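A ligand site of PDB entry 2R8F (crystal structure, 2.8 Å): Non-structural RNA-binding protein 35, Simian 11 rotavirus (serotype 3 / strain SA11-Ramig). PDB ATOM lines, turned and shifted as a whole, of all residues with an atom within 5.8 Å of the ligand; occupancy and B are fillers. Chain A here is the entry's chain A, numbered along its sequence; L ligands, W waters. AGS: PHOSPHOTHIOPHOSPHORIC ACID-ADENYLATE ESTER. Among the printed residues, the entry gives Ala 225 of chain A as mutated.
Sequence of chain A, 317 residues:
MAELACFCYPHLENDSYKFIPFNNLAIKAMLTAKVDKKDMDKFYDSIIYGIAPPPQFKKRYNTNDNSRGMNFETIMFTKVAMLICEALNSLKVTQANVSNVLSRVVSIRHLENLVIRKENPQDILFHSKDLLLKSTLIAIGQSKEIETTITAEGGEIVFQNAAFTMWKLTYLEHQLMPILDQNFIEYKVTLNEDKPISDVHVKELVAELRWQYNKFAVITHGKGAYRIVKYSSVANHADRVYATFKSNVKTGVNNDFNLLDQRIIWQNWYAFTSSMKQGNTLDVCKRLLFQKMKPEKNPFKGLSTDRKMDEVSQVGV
Water W5 lies within hydrogen-bond range of O2A of the ligand (2.6 Å) and NH1 of Arg 109 (3.1 Å). Water W7 lies within hydrogen-bond range of an oxygen (O1A) of the ligand (2.6 Å) and the side-chain hydroxyl of Ser 107 (2.8 Å). Water W8 lies within hydrogen-bond range of the side-chain carboxylate (OE2) of Glu 153 (2.8 Å), an oxygen (O1B) of the ligand (2.9 Å), the side-chain hydroxyl (OH) of Tyr 171 (3.0 Å) and the guanidinium group (NH2) of Arg 227 (3.1 Å). Water W1 lies within hydrogen-bond range of N of Lys 223 (3.0 Å), O2G of the ligand (3.1 Å) and O of Ala 225 (3.2 Å).
Residues that only touch the ligand: Ser 107 (3.9 Å) and Arg 240 (3.4 Å). Hydrophobic or aromatic side chains that line the ligand: His 221.
OG1 of Thr 244 sits at hydrogen-bond distance from O of Arg 240, at 2.7 Å. OE2 of Glu 153 lies within salt-bridge range of NH1 of Arg 227 (3.6 Å). NH2 of Arg 227 lies within hydrogen-bond range of OH of Tyr 171 (3.3 Å). NE of Arg 227 is in salt-bridge range of OE2 of Glu 186. The side-chain amino group of Lys 188 is in salt-bridge range of the side-chain carboxylate of Glu 153, at 2.7 Å. The side-chain carboxylate (OE2) of Glu 147 is in salt-bridge range of the side-chain amino group (NZ) of Lys 188. The guanidinium group (NE) of Arg 109 is in hydrogen-bond range of the backbone carbonyl oxygen (O) of Met 177 (3.4 Å). The backbone NH (N) of His 110 lies within hydrogen-bond range of the side-chain hydroxyl (OG) of Ser 107, at 3.3 Å.
NZ of Lys 223 lies within salt-bridge range of O2B of the ligand, 2.7 Å away. OG1 of Thr 244 is in hydrogen-bond range of O3' of the ligand (2.7 Å). NH2 of Arg 227 lies within salt-bridge range of O1A of the ligand (3.1 Å). O3B of the ligand lies within hydrogen-bond range of ND1 of His 221, 3.0 Å away. NZ of Lys 188 sits at hydrogen-bond distance from O3G of the ligand, 3.2 Å away. NH2 of Arg 109 lies within hydrogen-bond range of N1 of the ligand (3.3 Å).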
ATOM      1  N   ARG A  68     -23.939  19.100 -13.897  1.00  0.00           N
ATOM      2  CA  ARG A  68     -24.030  17.823 -14.584  1.00  0.00           C
ATOM      3  C   ARG A  68     -24.684  17.990 -15.963  1.00  0.00           C
ATOM      4  O   ARG A  68     -24.920  17.011 -16.665  1.00  0.00           O
ATOM      5  CB  ARG A  68     -24.835  16.853 -13.707  1.00  0.00           C
ATOM      6  CG  ARG A  68     -24.794  15.389 -14.125  1.00  0.00           C
ATOM      7  CD  ARG A  68     -24.664  14.450 -12.918  1.00  0.00           C
ATOM      8  NE  ARG A  68     -23.358  14.534 -12.276  1.00  0.00           N
ATOM      9  CZ  ARG A  68     -22.949  13.756 -11.271  1.00  0.00           C
ATOM     10  NH1 ARG A  68     -23.750  12.811 -10.784  1.00  0.00           N
ATOM     11  NH2 ARG A  68     -21.732  13.909 -10.746  1.00  0.00           N
ATOM     12  N   SER A 107     -24.499  12.610 -28.519  1.00  0.00           N
ATOM     13  CA  SER A 107     -23.330  13.041 -27.777  1.00  0.00           C
ATOM     14  C   SER A 107     -23.004  14.499 -28.080  1.00  0.00           C
ATOM     15  O   SER A 107     -22.696  14.872 -29.213  1.00  0.00           O
ATOM     16  CB  SER A 107     -22.110  12.170 -28.124  1.00  0.00           C
ATOM     17  OG  SER A 107     -20.919  12.714 -27.582  1.00  0.00           O
ATOM     18  N   ARG A 109     -20.418  16.260 -26.881  1.00  0.00           N
ATOM     19  CA  ARG A 109     -19.013  16.439 -27.181  1.00  0.00           C
ATOM     20  C   ARG A 109     -18.724  16.137 -28.647  1.00  0.00           C
ATOM     21  O   ARG A 109     -17.890  16.788 -29.263  1.00  0.00           O
ATOM     22  CB  ARG A 109     -18.143  15.561 -26.279  1.00  0.00           C
ATOM     23  CG  ARG A 109     -18.266  15.941 -24.821  1.00  0.00           C
ATOM     24  CD  ARG A 109     -17.378  15.110 -23.926  1.00  0.00           C
ATOM     25  NE  ARG A 109     -17.919  15.079 -22.572  1.00  0.00           N
ATOM     26  CZ  ARG A 109     -18.919  14.298 -22.182  1.00  0.00           C
ATOM     27  NH1 ARG A 109     -19.489  13.465 -23.043  1.00  0.00           N
ATOM     28  NH2 ARG A 109     -19.366  14.362 -20.931  1.00  0.00           N
ATOM     29  N   HIS A 110     -19.442  15.153 -29.194  1.00  0.00           N
ATOM     30  CA  HIS A 110     -19.275  14.786 -30.596  1.00  0.00           C
ATOM     31  C   HIS A 110     -19.755  15.925 -31.526  1.00  0.00           C
ATOM     32  O   HIS A 110     -19.165  16.186 -32.583  1.00  0.00           O
ATOM     33  CB  HIS A 110     -20.059  13.501 -30.898  1.00  0.00           C
ATOM     34  CG  HIS A 110     -19.689  12.829 -32.180  1.00  0.00           C
ATOM     35  ND1 HIS A 110     -19.740  13.465 -33.406  1.00  0.00           N
ATOM     36  CD2 HIS A 110     -19.306  11.561 -32.443  1.00  0.00           C
ATOM     37  CE1 HIS A 110     -19.399  12.622 -34.362  1.00  0.00           C
ATOM     38  NE2 HIS A 110     -19.127  11.449 -33.800  1.00  0.00           N
ATOM     39  N   GLU A 147     -18.799   6.023 -39.009  1.00  0.00           N
ATOM     40  CA  GLU A 147     -17.847   7.109 -38.894  1.00  0.00           C
ATOM     41  C   GLU A 147     -16.462   6.618 -39.285  1.00  0.00           C
ATOM     42  O   GLU A 147     -15.968   5.624 -38.766  1.00  0.00           O
ATOM     43  CB  GLU A 147     -17.810   7.617 -37.448  1.00  0.00           C
ATOM     44  CG  GLU A 147     -16.959   8.866 -37.266  1.00  0.00           C
ATOM     45  CD  GLU A 147     -16.783   9.248 -35.802  1.00  0.00           C
ATOM     46  OE1 GLU A 147     -17.699   8.982 -35.000  1.00  0.00           O
ATOM     47  OE2 GLU A 147     -15.731   9.832 -35.466  1.00  0.00           O
ATOM     48  N   GLU A 153     -15.237  12.816 -35.589  1.00  0.00           N
ATOM     49  CA  GLU A 153     -15.558  13.988 -34.783  1.00  0.00           C
ATOM     50  C   GLU A 153     -14.332  14.886 -34.672  1.00  0.00           C
ATOM     51  O   GLU A 153     -14.438  16.034 -34.239  1.00  0.00           O
ATOM     52  CB  GLU A 153     -16.019  13.559 -33.396  1.00  0.00           C
ATOM     53  CG  GLU A 153     -15.007  12.779 -32.613  1.00  0.00           C
ATOM     54  CD  GLU A 153     -15.513  12.396 -31.244  1.00  0.00           C
ATOM     55  OE1 GLU A 153     -15.815  13.305 -30.443  1.00  0.00           O
ATOM     56  OE2 GLU A 153     -15.606  11.188 -30.963  1.00  0.00           O
ATOM     57  N   TYR A 171     -11.860  16.968 -25.282  1.00  0.00           N
ATOM     58  CA  TYR A 171     -13.015  17.252 -24.437  1.00  0.00           C
ATOM     59  C   TYR A 171     -12.747  18.224 -23.284  1.00  0.00           C
ATOM     60  O   TYR A 171     -13.636  19.022 -22.919  1.00  0.00           O
ATOM     61  CB  TYR A 171     -13.576  15.934 -23.868  1.00  0.00           C
ATOM     62  CG  TYR A 171     -14.120  14.979 -24.901  1.00  0.00           C
ATOM     63  CD1 TYR A 171     -14.177  13.612 -24.639  1.00  0.00           C
ATOM     64  CD2 TYR A 171     -14.579  15.437 -26.140  1.00  0.00           C
ATOM     65  CE1 TYR A 171     -14.669  12.710 -25.582  1.00  0.00           C
ATOM     66  CE2 TYR A 171     -15.086  14.555 -27.086  1.00  0.00           C
ATOM     67  CZ  TYR A 171     -15.123  13.195 -26.799  1.00  0.00           C
ATOM     68  OH  TYR A 171     -15.620  12.320 -27.739  1.00  0.00           O
ATOM     69  N   MET A 177     -19.973  21.268 -23.208  1.00  0.00           N
ATOM     70  CA  MET A 177     -20.040  20.322 -22.110  1.00  0.00           C
ATOM     71  C   MET A 177     -18.752  19.549 -21.984  1.00  0.00           C
ATOM     72  O   MET A 177     -18.695  18.363 -22.312  1.00  0.00           O
ATOM     73  CB  MET A 177     -21.190  19.333 -22.303  1.00  0.00           C
ATOM     74  CG  MET A 177     -21.485  18.503 -21.059  1.00  0.00           C
ATOM     75  SD  MET A 177     -22.946  17.464 -21.151  1.00  0.00           S
ATOM     76  CE  MET A 177     -22.203  15.857 -21.293  1.00  0.00           C
ATOM     77  N   GLU A 186      -7.965  10.565 -23.599  1.00  0.00           N
ATOM     78  CA  GLU A 186      -8.610   9.530 -24.398  1.00  0.00           C
ATOM     79  C   GLU A 186      -8.339   9.762 -25.875  1.00  0.00           C
ATOM     80  O   GLU A 186      -8.304  10.901 -26.324  1.00  0.00           O
ATOM     81  CB  GLU A 186     -10.118   9.527 -24.120  1.00  0.00           C
ATOM     82  CG  GLU A 186     -10.856   8.320 -24.649  1.00  0.00           C
ATOM     83  CD  GLU A 186     -12.283   8.227 -24.124  1.00  0.00           C
ATOM     84  OE1 GLU A 186     -12.467   8.131 -22.882  1.00  0.00           O
ATOM     85  OE2 GLU A 186     -13.240   8.237 -24.932  1.00  0.00           O
ATOM     86  N   LYS A 188      -9.083   8.320 -30.119  1.00  0.00           N
ATOM     87  CA  LYS A 188      -9.989   7.589 -30.993  1.00  0.00           C
ATOM     88  C   LYS A 188      -9.254   7.249 -32.274  1.00  0.00           C
ATOM     89  O   LYS A 188      -8.521   8.080 -32.799  1.00  0.00           O
ATOM     90  CB  LYS A 188     -11.195   8.491 -31.305  1.00  0.00           C
ATOM     91  CG  LYS A 188     -12.293   7.857 -32.111  1.00  0.00           C
ATOM     92  CD  LYS A 188     -13.424   8.849 -32.276  1.00  0.00           C
ATOM     93  CE  LYS A 188     -14.670   8.212 -32.839  1.00  0.00           C
ATOM     94  NZ  LYS A 188     -15.841   9.121 -32.689  1.00  0.00           N
ATOM     95  N   THR A 220     -13.419  -0.661 -27.933  1.00  0.00           N
ATOM     96  CA  THR A 220     -14.318  -0.136 -28.968  1.00  0.00           C
ATOM     97  C   THR A 220     -15.744  -0.148 -28.450  1.00  0.00           C
ATOM     98  O   THR A 220     -16.094  -1.019 -27.659  1.00  0.00           O
ATOM     99  CB  THR A 220     -14.286  -0.999 -30.247  1.00  0.00           C
ATOM    100  OG1 THR A 220     -15.330  -0.577 -31.139  1.00  0.00           O
ATOM    101  CG2 THR A 220     -14.496  -2.472 -29.918  1.00  0.00           C
ATOM    102  N   HIS A 221     -16.544   0.813 -28.881  1.00  0.00           N
ATOM    103  CA  HIS A 221     -17.944   0.851 -28.477  1.00  0.00           C
ATOM    104  C   HIS A 221     -18.753   0.169 -29.574  1.00  0.00           C
ATOM    105  O   HIS A 221     -19.984   0.192 -29.562  1.00  0.00           O
ATOM    106  CB  HIS A 221     -18.426   2.285 -28.263  1.00  0.00           C
ATOM    107  CG  HIS A 221     -17.838   2.937 -27.056  1.00  0.00           C
ATOM    108  ND1 HIS A 221     -18.133   4.240 -26.691  1.00  0.00           N
ATOM    109  CD2 HIS A 221     -16.950   2.481 -26.148  1.00  0.00           C
ATOM    110  CE1 HIS A 221     -17.448   4.550 -25.607  1.00  0.00           C
ATOM    111  NE2 HIS A 221     -16.727   3.508 -25.252  1.00  0.00           N
ATOM    112  N   LYS A 223     -18.985   0.812 -32.968  1.00  0.00           N
ATOM    113  CA  LYS A 223     -19.558   1.498 -34.105  1.00  0.00           C
ATOM    114  C   LYS A 223     -18.540   1.726 -35.219  1.00  0.00           C
ATOM    115  O   LYS A 223     -18.729   2.575 -36.089  1.00  0.00           O
ATOM    116  CB  LYS A 223     -20.190   2.812 -33.643  1.00  0.00           C
ATOM    117  CG  LYS A 223     -21.271   2.610 -32.573  1.00  0.00           C
ATOM    118  CD  LYS A 223     -21.807   3.944 -32.048  1.00  0.00           C
ATOM    119  CE  LYS A 223     -22.640   3.756 -30.771  1.00  0.00           C
ATOM    120  NZ  LYS A 223     -23.148   5.068 -30.218  1.00  0.00           N
ATOM    121  N   ALA A 225     -14.908   2.195 -34.676  1.00  0.00           N
ATOM    122  CA  ALA A 225     -13.655   2.879 -34.366  1.00  0.00           C
ATOM    123  C   ALA A 225     -13.074   2.406 -33.047  1.00  0.00           C
ATOM    124  O   ALA A 225     -13.808   1.973 -32.150  1.00  0.00           O
ATOM    125  CB  ALA A 225     -13.876   4.364 -34.316  1.00  0.00           C
ATOM    126  N   TYR A 226     -11.753   2.471 -32.930  1.00  0.00           N
ATOM    127  CA  TYR A 226     -11.101   2.065 -31.692  1.00  0.00           C
ATOM    128  C   TYR A 226     -11.104   3.211 -30.674  1.00  0.00           C
ATOM    129  O   TYR A 226     -11.036   4.386 -31.047  1.00  0.00           O
ATOM    130  CB  TYR A 226      -9.662   1.621 -31.961  1.00  0.00           C
ATOM    131  CG  TYR A 226      -9.577   0.456 -32.911  1.00  0.00           C
ATOM    132  CD1 TYR A 226      -9.381   0.667 -34.278  1.00  0.00           C
ATOM    133  CD2 TYR A 226      -9.715  -0.845 -32.450  1.00  0.00           C
ATOM    134  CE1 TYR A 226      -9.343  -0.394 -35.161  1.00  0.00           C
ATOM    135  CE2 TYR A 226      -9.686  -1.922 -33.328  1.00  0.00           C
ATOM    136  CZ  TYR A 226      -9.495  -1.693 -34.681  1.00  0.00           C
ATOM    137  OH  TYR A 226      -9.462  -2.761 -35.561  1.00  0.00           O
ATOM    138  N   ARG A 227     -11.195   2.878 -29.395  1.00  0.00           N
ATOM    139  CA  ARG A 227     -11.193   3.884 -28.355  1.00  0.00           C
ATOM    140  C   ARG A 227     -10.019   3.531 -27.450  1.00  0.00           C
ATOM    141  O   ARG A 227      -9.959   2.422 -26.904  1.00  0.00           O
ATOM    142  CB  ARG A 227     -12.510   3.837 -27.591  1.00  0.00           C
ATOM    143  CG  ARG A 227     -12.934   5.148 -26.946  1.00  0.00           C
ATOM    144  CD  ARG A 227     -13.734   6.031 -27.898  1.00  0.00           C
ATOM    145  NE  ARG A 227     -14.303   7.181 -27.196  1.00  0.00           N
ATOM    146  CZ  ARG A 227     -15.050   8.135 -27.760  1.00  0.00           C
ATOM    147  NH1 ARG A 227     -15.339   8.093 -29.058  1.00  0.00           N
ATOM    148  NH2 ARG A 227     -15.514   9.136 -27.022  1.00  0.00           N
ATOM    149  N   ARG A 240     -21.238   1.259 -19.656  1.00  0.00           N
ATOM    150  CA  ARG A 240     -21.947   2.066 -20.641  1.00  0.00           C
ATOM    151  C   ARG A 240     -22.258   1.310 -21.928  1.00  0.00           C
ATOM    152  O   ARG A 240     -23.315   1.510 -22.518  1.00  0.00           O
ATOM    153  CB  ARG A 240     -21.152   3.333 -20.965  1.00  0.00           C
ATOM    154  CG  ARG A 240     -20.782   4.135 -19.730  1.00  0.00           C
ATOM    155  CD  ARG A 240     -20.742   5.621 -20.033  1.00  0.00           C
ATOM    156  NE  ARG A 240     -19.763   5.967 -21.060  1.00  0.00           N
ATOM    157  CZ  ARG A 240     -18.453   5.953 -20.862  1.00  0.00           C
ATOM    158  NH1 ARG A 240     -17.945   5.619 -19.676  1.00  0.00           N
ATOM    159  NH2 ARG A 240     -17.635   6.298 -21.856  1.00  0.00           N
ATOM    160  N   VAL A 241     -21.343   0.451 -22.379  1.00  0.00           N
ATOM    161  CA  VAL A 241     -21.566  -0.307 -23.612  1.00  0.00           C
ATOM    162  C   VAL A 241     -22.596  -1.400 -23.387  1.00  0.00           C
ATOM    163  O   VAL A 241     -23.359  -1.744 -24.280  1.00  0.00           O
ATOM    164  CB  VAL A 241     -20.270  -0.964 -24.149  1.00  0.00           C
ATOM    165  CG1 VAL A 241     -19.205   0.084 -24.374  1.00  0.00           C
ATOM    166  CG2 VAL A 241     -19.787  -2.026 -23.193  1.00  0.00           C
ATOM    167  N   ALA A 243     -25.106  -1.358 -20.931  1.00  0.00           N
ATOM    168  CA  ALA A 243     -26.378  -0.661 -20.773  1.00  0.00           C
ATOM    169  C   ALA A 243     -26.964  -0.354 -22.146  1.00  0.00           C
ATOM    170  O   ALA A 243     -28.173  -0.502 -22.365  1.00  0.00           O
ATOM    171  CB  ALA A 243     -26.153   0.631 -19.998  1.00  0.00           C
ATOM    172  N   THR A 244     -26.104   0.071 -23.055  1.00  0.00           N
ATOM    173  CA  THR A 244     -26.508   0.405 -24.413  1.00  0.00           C
ATOM    174  C   THR A 244     -27.001  -0.839 -25.161  1.00  0.00           C
ATOM    175  O   THR A 244     -28.047  -0.803 -25.803  1.00  0.00           O
ATOM    176  CB  THR A 244     -25.336   1.012 -25.198  1.00  0.00           C
ATOM    177  OG1 THR A 244     -24.926   2.230 -24.555  1.00  0.00           O
ATOM    178  CG2 THR A 244     -25.738   1.313 -26.628  1.00  0.00           C
HETATM  179  PG  AGS L   1     -17.886   6.110 -30.236  1.00  0.00           P
HETATM  180  S1G AGS L   1     -16.084   5.131 -29.997  1.00  0.00           S
HETATM  181  O2G AGS L   1     -18.598   5.371 -31.287  1.00  0.00           O
HETATM  182  O3G AGS L   1     -17.680   7.524 -30.658  1.00  0.00           O
HETATM  183  PB  AGS L   1     -20.003   7.103 -28.578  1.00  0.00           P
HETATM  184  O1B AGS L   1     -19.767   8.560 -28.820  1.00  0.00           O
HETATM  185  O2B AGS L   1     -21.118   6.580 -29.368  1.00  0.00           O
HETATM  186  O3B AGS L   1     -18.756   6.139 -28.901  1.00  0.00           O
HETATM  187  PA  AGS L   1     -19.852   7.986 -25.967  1.00  0.00           P
HETATM  188  O1A AGS L   1     -18.433   8.407 -26.179  1.00  0.00           O
HETATM  189  O2A AGS L   1     -20.818   9.116 -26.008  1.00  0.00           O
HETATM  190  O3A AGS L   1     -20.348   6.903 -27.058  1.00  0.00           O
HETATM  191  O5' AGS L   1     -20.082   7.266 -24.522  1.00  0.00           O
HETATM  192  C5' AGS L   1     -20.774   6.039 -24.310  1.00  0.00           C
HETATM  193  C4' AGS L   1     -22.275   6.327 -24.269  1.00  0.00           C
HETATM  194  O4' AGS L   1     -22.519   7.575 -23.592  1.00  0.00           O
HETATM  195  C3' AGS L   1     -23.156   5.326 -23.500  1.00  0.00           C
HETATM  196  O3' AGS L   1     -24.145   4.849 -24.415  1.00  0.00           O
HETATM  197  C2' AGS L   1     -23.830   6.135 -22.475  1.00  0.00           C
HETATM  198  O2' AGS L   1     -24.060   5.310 -21.336  1.00  0.00           O
HETATM  199  C1' AGS L   1     -22.873   7.222 -22.260  1.00  0.00           C
HETATM  200  N9  AGS L   1     -23.191   8.382 -21.318  1.00  0.00           N
HETATM  201  C8  AGS L   1     -24.322   8.661 -20.658  1.00  0.00           C
HETATM  202  N7  AGS L   1     -24.109   9.801 -19.944  1.00  0.00           N
HETATM  203  C5  AGS L   1     -22.852  10.256 -20.168  1.00  0.00           C
HETATM  204  C6  AGS L   1     -22.063  11.347 -19.732  1.00  0.00           C
HETATM  205  N6  AGS L   1     -22.507  12.306 -18.882  1.00  0.00           N
HETATM  206  N1  AGS L   1     -20.781  11.478 -20.174  1.00  0.00           N
HETATM  207  C2  AGS L   1     -20.244  10.570 -21.025  1.00  0.00           C
HETATM  208  N3  AGS L   1     -20.983   9.526 -21.440  1.00  0.00           N
HETATM  209  C4  AGS L   1     -22.284   9.340 -21.026  1.00  0.00           C
HETATM  210  O   HOH W   1     -16.933   2.822 -32.039  1.00  0.00           O
HETATM  211  O   HOH W   2     -22.318   9.086 -29.749  1.00  0.00           O
HETATM  212  O   HOH W   3     -24.294   9.683 -25.410  1.00  0.00           O
HETATM  213  O   HOH W   4     -18.070  10.157 -18.996  1.00  0.00           O
HETATM  214  O   HOH W   5     -21.051  11.089 -24.337  1.00  0.00           O
HETATM  215  O   HOH W   6     -21.857   4.480 -26.665  1.00  0.00           O
HETATM  216  O   HOH W   7     -18.836  10.885 -26.983  1.00  0.00           O
HETATM  217  O   HOH W   8     -17.554  10.384 -29.071  1.00  0.00           O
